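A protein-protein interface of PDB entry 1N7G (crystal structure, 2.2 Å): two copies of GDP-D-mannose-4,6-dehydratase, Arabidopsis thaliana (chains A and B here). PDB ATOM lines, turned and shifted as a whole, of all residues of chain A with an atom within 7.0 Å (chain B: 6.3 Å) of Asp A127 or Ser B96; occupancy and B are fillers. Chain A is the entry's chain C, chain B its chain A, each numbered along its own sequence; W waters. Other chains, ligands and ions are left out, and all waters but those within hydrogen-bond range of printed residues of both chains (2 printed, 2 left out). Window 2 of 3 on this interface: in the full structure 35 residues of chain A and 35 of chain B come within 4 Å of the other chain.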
ATOM      1  N   SER A 122      25.010 -35.866  -3.386  1.00  0.00           N
ATOM      2  CA  SER A 122      25.509 -34.570  -2.933  1.00  0.00           C
ATOM      3  C   SER A 122      25.696 -33.578  -4.080  1.00  0.00           C
ATOM      4  O   SER A 122      25.620 -32.365  -3.869  1.00  0.00           O
ATOM      5  CB  SER A 122      26.813 -34.727  -2.132  1.00  0.00           C
ATOM      6  OG  SER A 122      27.928 -35.015  -2.957  1.00  0.00           O
ATOM      7  N   GLU A 124      23.657 -33.299  -6.454  1.00  0.00           N
ATOM      8  CA  GLU A 124      22.293 -32.863  -6.771  1.00  0.00           C
ATOM      9  C   GLU A 124      21.710 -31.871  -5.765  1.00  0.00           C
ATOM     10  O   GLU A 124      21.003 -30.934  -6.143  1.00  0.00           O
ATOM     11  CB  GLU A 124      21.366 -34.068  -6.855  1.00  0.00           C
ATOM     12  CG  GLU A 124      21.852 -35.169  -7.760  1.00  0.00           C
ATOM     13  CD  GLU A 124      20.746 -35.694  -8.635  1.00  0.00           C
ATOM     14  OE1 GLU A 124      20.459 -35.052  -9.667  1.00  0.00           O
ATOM     15  OE2 GLU A 124      20.152 -36.733  -8.281  1.00  0.00           O
ATOM     16  N   ILE A 125      21.995 -32.105  -4.484  1.00  0.00           N
ATOM     17  CA  ILE A 125      21.534 -31.246  -3.395  1.00  0.00           C
ATOM     18  C   ILE A 125      22.732 -30.792  -2.559  1.00  0.00           C
ATOM     19  O   ILE A 125      22.837 -31.119  -1.377  1.00  0.00           O
ATOM     20  CB  ILE A 125      20.548 -31.989  -2.466  1.00  0.00           C
ATOM     21  CG1 ILE A 125      21.099 -33.377  -2.129  1.00  0.00           C
ATOM     22  CG2 ILE A 125      19.176 -32.068  -3.113  1.00  0.00           C
ATOM     23  CD1 ILE A 125      20.266 -34.141  -1.137  1.00  0.00           C
ATOM     24  N   PRO A 126      23.644 -30.014  -3.166  1.00  0.00           N
ATOM     25  CA  PRO A 126      24.835 -29.529  -2.456  1.00  0.00           C
ATOM     26  C   PRO A 126      24.546 -28.648  -1.239  1.00  0.00           C
ATOM     27  O   PRO A 126      25.143 -28.837  -0.178  1.00  0.00           O
ATOM     28  CB  PRO A 126      25.612 -28.797  -3.550  1.00  0.00           C
ATOM     29  CG  PRO A 126      24.522 -28.295  -4.456  1.00  0.00           C
ATOM     30  CD  PRO A 126      23.592 -29.480  -4.539  1.00  0.00           C
ATOM     31  N   ASP A 127      23.636 -27.692  -1.398  1.00  0.00           N
ATOM     32  CA  ASP A 127      23.274 -26.792  -0.312  1.00  0.00           C
ATOM     33  C   ASP A 127      22.806 -27.558   0.930  1.00  0.00           C
ATOM     34  O   ASP A 127      23.330 -27.354   2.024  1.00  0.00           O
ATOM     35  CB  ASP A 127      22.189 -25.812  -0.779  1.00  0.00           C
ATOM     36  CG  ASP A 127      22.687 -24.853  -1.867  1.00  0.00           C
ATOM     37  OD1 ASP A 127      21.868 -24.092  -2.427  1.00  0.00           O
ATOM     38  OD2 ASP A 127      23.901 -24.851  -2.164  1.00  0.00           O
ATOM     39  N   TYR A 128      21.824 -28.436   0.760  1.00  0.00           N
ATOM     40  CA  TYR A 128      21.314 -29.228   1.875  1.00  0.00           C
ATOM     41  C   TYR A 128      22.416 -30.106   2.477  1.00  0.00           C
ATOM     42  O   TYR A 128      22.559 -30.196   3.696  1.00  0.00           O
ATOM     43  CB  TYR A 128      20.153 -30.121   1.412  1.00  0.00           C
ATOM     44  CG  TYR A 128      19.673 -31.063   2.484  1.00  0.00           C
ATOM     45  CD1 TYR A 128      18.768 -30.643   3.461  1.00  0.00           C
ATOM     46  CD2 TYR A 128      20.199 -32.354   2.579  1.00  0.00           C
ATOM     47  CE1 TYR A 128      18.402 -31.487   4.516  1.00  0.00           C
ATOM     48  CE2 TYR A 128      19.844 -33.202   3.629  1.00  0.00           C
ATOM     49  CZ  TYR A 128      18.948 -32.763   4.593  1.00  0.00           C
ATOM     50  OH  TYR A 128      18.632 -33.597   5.637  1.00  0.00           O
ATOM     51  N   THR A 129      23.188 -30.759   1.615  1.00  0.00           N
ATOM     52  CA  THR A 129      24.261 -31.635   2.061  1.00  0.00           C
ATOM     53  C   THR A 129      25.251 -30.873   2.929  1.00  0.00           C
ATOM     54  O   THR A 129      25.607 -31.325   4.012  1.00  0.00           O
ATOM     55  CB  THR A 129      25.014 -32.260   0.858  1.00  0.00           C
ATOM     56  OG1 THR A 129      24.109 -33.067   0.095  1.00  0.00           O
ATOM     57  CG2 THR A 129      26.181 -33.122   1.332  1.00  0.00           C
ATOM     58  N   ALA A 130      25.688 -29.713   2.455  1.00  0.00           N
ATOM     59  CA  ALA A 130      26.639 -28.908   3.201  1.00  0.00           C
ATOM     60  C   ALA A 130      26.059 -28.487   4.548  1.00  0.00           C
ATOM     61  O   ALA A 130      26.772 -28.456   5.545  1.00  0.00           O
ATOM     62  CB  ALA A 130      27.034 -27.672   2.394  1.00  0.00           C
ATOM     63  N   ASP A 131      24.765 -28.174   4.572  1.00  0.00           N
ATOM     64  CA  ASP A 131      24.115 -27.740   5.802  1.00  0.00           C
ATOM     65  C   ASP A 131      24.027 -28.839   6.856  1.00  0.00           C
ATOM     66  O   ASP A 131      24.047 -28.559   8.053  1.00  0.00           O
ATOM     67  CB  ASP A 131      22.713 -27.196   5.503  1.00  0.00           C
ATOM     68  CG  ASP A 131      22.169 -26.341   6.631  1.00  0.00           C
ATOM     69  OD1 ASP A 131      22.884 -25.424   7.083  1.00  0.00           O
ATOM     70  OD2 ASP A 131      21.024 -26.574   7.062  1.00  0.00           O
ATOM     71  N   VAL A 132      23.925 -30.086   6.414  1.00  0.00           N
ATOM     72  CA  VAL A 132      23.849 -31.204   7.339  1.00  0.00           C
ATOM     73  C   VAL A 132      25.236 -31.734   7.709  1.00  0.00           C
ATOM     74  O   VAL A 132      25.546 -31.928   8.892  1.00  0.00           O
ATOM     75  CB  VAL A 132      23.036 -32.372   6.740  1.00  0.00           C
ATOM     76  CG1 VAL A 132      23.003 -33.543   7.721  1.00  0.00           C
ATOM     77  CG2 VAL A 132      21.632 -31.906   6.414  1.00  0.00           C
ATOM     78  N   PRO A 184      30.721 -32.168  -3.257  1.00  0.00           N
ATOM     79  CA  PRO A 184      30.239 -31.270  -2.205  1.00  0.00           C
ATOM     80  C   PRO A 184      30.253 -32.003  -0.870  1.00  0.00           C
ATOM     81  O   PRO A 184      30.604 -31.429   0.157  1.00  0.00           O
ATOM     82  CB  PRO A 184      28.833 -30.923  -2.673  1.00  0.00           C
ATOM     83  CG  PRO A 184      29.000 -30.898  -4.171  1.00  0.00           C
ATOM     84  CD  PRO A 184      29.803 -32.160  -4.411  1.00  0.00           C
ATOM     85  N   SER A 188      32.366 -30.918   2.347  1.00  0.00           N
ATOM     86  CA  SER A 188      31.647 -30.696   3.597  1.00  0.00           C
ATOM     87  C   SER A 188      32.225 -31.525   4.744  1.00  0.00           C
ATOM     88  O   SER A 188      32.257 -31.071   5.887  1.00  0.00           O
ATOM     89  CB  SER A 188      30.157 -30.992   3.416  1.00  0.00           C
ATOM     90  OG  SER A 188      29.566 -30.023   2.565  1.00  0.00           O
ATOM     91  N   ASP B  94      15.925 -26.303   1.242  1.00  0.00           N
ATOM     92  CA  ASP B  94      16.958 -25.981   0.257  1.00  0.00           C
ATOM     93  C   ASP B  94      16.310 -25.332  -0.964  1.00  0.00           C
ATOM     94  O   ASP B  94      15.851 -26.020  -1.881  1.00  0.00           O
ATOM     95  CB  ASP B  94      17.708 -27.257  -0.155  1.00  0.00           C
ATOM     96  CG  ASP B  94      18.818 -26.995  -1.171  1.00  0.00           C
ATOM     97  OD1 ASP B  94      19.598 -27.935  -1.456  1.00  0.00           O
ATOM     98  OD2 ASP B  94      18.916 -25.861  -1.687  1.00  0.00           O
ATOM     99  N   ALA B  95      16.281 -24.002  -0.960  1.00  0.00           N
ATOM    100  CA  ALA B  95      15.690 -23.226  -2.043  1.00  0.00           C
ATOM    101  C   ALA B  95      16.282 -23.587  -3.399  1.00  0.00           C
ATOM    102  O   ALA B  95      15.554 -23.700  -4.383  1.00  0.00           O
ATOM    103  CB  ALA B  95      15.865 -21.723  -1.770  1.00  0.00           C
ATOM    104  N   SER B  96      17.600 -23.761  -3.450  1.00  0.00           N
ATOM    105  CA  SER B  96      18.273 -24.122  -4.694  1.00  0.00           C
ATOM    106  C   SER B  96      17.672 -25.376  -5.289  1.00  0.00           C
ATOM    107  O   SER B  96      17.309 -25.398  -6.457  1.00  0.00           O
ATOM    108  CB  SER B  96      19.763 -24.379  -4.464  1.00  0.00           C
ATOM    109  OG  SER B  96      20.449 -23.187  -4.156  1.00  0.00           O
ATOM    110  N   SER B  97      17.579 -26.421  -4.475  1.00  0.00           N
ATOM    111  CA  SER B  97      17.045 -27.695  -4.928  1.00  0.00           C
ATOM    112  C   SER B  97      15.670 -27.533  -5.542  1.00  0.00           C
ATOM    113  O   SER B  97      15.342 -28.207  -6.512  1.00  0.00           O
ATOM    114  CB  SER B  97      16.972 -28.700  -3.769  1.00  0.00           C
ATOM    115  OG  SER B  97      15.863 -28.445  -2.923  1.00  0.00           O
ATOM    116  N   LEU B  98      14.863 -26.639  -4.981  1.00  0.00           N
ATOM    117  CA  LEU B  98      13.518 -26.429  -5.499  1.00  0.00           C
ATOM    118  C   LEU B  98      13.537 -25.815  -6.896  1.00  0.00           C
ATOM    119  O   LEU B  98      13.055 -26.417  -7.856  1.00  0.00           O
ATOM    120  CB  LEU B  98      12.728 -25.522  -4.560  1.00  0.00           C
ATOM    121  CG  LEU B  98      12.605 -25.990  -3.109  1.00  0.00           C
ATOM    122  CD1 LEU B  98      11.618 -25.078  -2.389  1.00  0.00           C
ATOM    123  CD2 LEU B  98      12.143 -27.438  -3.059  1.00  0.00           C
ATOM    124  N   ARG B  99      14.099 -24.615  -6.997  1.00  0.00           N
ATOM    125  CA  ARG B  99      14.184 -23.892  -8.257  1.00  0.00           C
ATOM    126  C   ARG B  99      14.836 -24.751  -9.337  1.00  0.00           C
ATOM    127  O   ARG B  99      14.421 -24.732 -10.498  1.00  0.00           O
ATOM    128  CB  ARG B  99      14.988 -22.602  -8.056  1.00  0.00           C
ATOM    129  CG  ARG B  99      15.168 -21.757  -9.304  1.00  0.00           C
ATOM    130  CD  ARG B  99      13.836 -21.261  -9.853  1.00  0.00           C
ATOM    131  NE  ARG B  99      14.010 -20.604 -11.145  1.00  0.00           N
ATOM    132  CZ  ARG B  99      14.578 -19.415 -11.308  1.00  0.00           C
ATOM    133  NH1 ARG B  99      15.025 -18.743 -10.255  1.00  0.00           N
ATOM    134  NH2 ARG B  99      14.711 -18.904 -12.526  1.00  0.00           N
ATOM    135  N   ARG B 100      15.854 -25.507  -8.945  1.00  0.00           N
ATOM    136  CA  ARG B 100      16.575 -26.367  -9.872  1.00  0.00           C
ATOM    137  C   ARG B 100      15.612 -27.252 -10.652  1.00  0.00           C
ATOM    138  O   ARG B 100      15.562 -27.197 -11.881  1.00  0.00           O
ATOM    139  CB  ARG B 100      17.579 -27.229  -9.103  1.00  0.00           C
ATOM    140  CG  ARG B 100      18.367 -28.216  -9.951  1.00  0.00           C
ATOM    141  CD  ARG B 100      19.593 -28.705  -9.191  1.00  0.00           C
ATOM    142  NE  ARG B 100      20.309 -29.777  -9.878  1.00  0.00           N
ATOM    143  CZ  ARG B 100      21.547 -30.161  -9.571  1.00  0.00           C
ATOM    144  NH1 ARG B 100      22.125 -31.150 -10.243  1.00  0.00           N
ATOM    145  NH2 ARG B 100      22.213 -29.549  -8.601  1.00  0.00           N
ATOM    146  N   TRP B 101      14.834 -28.053  -9.936  1.00  0.00           N
ATOM    147  CA  TRP B 101      13.895 -28.947 -10.586  1.00  0.00           C
ATOM    148  C   TRP B 101      12.747 -28.248 -11.290  1.00  0.00           C
ATOM    149  O   TRP B 101      12.212 -28.771 -12.260  1.00  0.00           O
ATOM    150  CB  TRP B 101      13.378 -29.971  -9.579  1.00  0.00           C
ATOM    151  CG  TRP B 101      14.464 -30.904  -9.200  1.00  0.00           C
ATOM    152  CD1 TRP B 101      15.015 -31.074  -7.963  1.00  0.00           C
ATOM    153  CD2 TRP B 101      15.198 -31.754 -10.088  1.00  0.00           C
ATOM    154  NE1 TRP B 101      16.053 -31.975  -8.027  1.00  0.00           N
ATOM    155  CE2 TRP B 101      16.188 -32.407  -9.319  1.00  0.00           C
ATOM    156  CE3 TRP B 101      15.118 -32.024 -11.461  1.00  0.00           C
ATOM    157  CZ2 TRP B 101      17.095 -33.317  -9.879  1.00  0.00           C
ATOM    158  CZ3 TRP B 101      16.021 -32.930 -12.020  1.00  0.00           C
ATOM    159  CH2 TRP B 101      16.997 -33.564 -11.227  1.00  0.00           C
HETATM  160  O   HOH W   1      19.844 -23.352  -1.129  1.00  0.00           O
HETATM  161  O   HOH W   2      21.422 -27.673  -3.366  1.00  0.00           O
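The side-chain carboxylate of Asp B94 is in hydrogen-bond range of the backbone NH of Ser B96, at 3.0 Å.
OG of Ser B97 lies within hydrogen-bond range of O of Asp B94 (2.6 Å).
Among the printed residues, pairs that only touch across the chains: Asp A127 with Asp B94 (3.4 Å) and Glu A124 with Trp B101 (3.8 Å).
No position is printed for both chains.
Of the 5 pairs that touch across the chains among the printed residues, none has its exchanged pair printed and touching as well.
The backbone NH (N) of Tyr A128 lies within hydrogen-bond range of the side-chain carboxylate (OD1) of Asp B94.
The side-chain carboxylate (OD1) of Asp A127 lies within hydrogen-bond range of the side-chain hydroxyl (OG) of Ser B96, at 2.4 Å.
The guanidinium group (NH2) of Arg B100 is in hydrogen-bond range of the backbone carbonyl oxygen (O) of Glu A124, 3.1 Å away.
Water W1 lies within hydrogen-bond range of OD1 of Asp A127 (2.5 Å), OD2 of Asp B94 (2.7 Å) and OG of Ser B96 (3.1 Å).
Water W2 lies within hydrogen-bond range of the side-chain carboxylate of Asp B94 (2.7 Å) and the backbone NH of Asp A127 (3.0 Å).
Of the 12 printed residues of chain A, 3 touch a printed residue of chain B.
Printed residues of chain A that touch a printed residue of chain B: Glu A124, Asp A127 and Tyr A128.
Hydrophobic or aromatic side chains of chain A within 4 Å of the printed part of chain B: Tyr A128.
Along chain A the printed residues that touch a printed residue of chain B span positions 124 to 128.
Among the printed residues, 5 pairs touch across the chains.
Of chain B, only Asp B94 (3.4 Å) and Ser B96 (2.4 Å) come within 4 Å of Asp A127.
Of the printed residues of chain B, Tyr A128 touches Asp B94 (3.2 Å).
Ser B96 touches just one residue of chain A: Asp A127.
Of the printed residues of chain A, Arg B100 touches Glu A124 (3.1 Å).
The nearest residue of chain B that does not touch Asp A127 is Ser B97 (5.3 Å).
The nearest residue of chain A that does not touch Ser B96 is Pro A126 (6.2 Å).
The nearest printed residue of chain A that does not touch Arg B100 is Pro A126 (4.3 Å).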
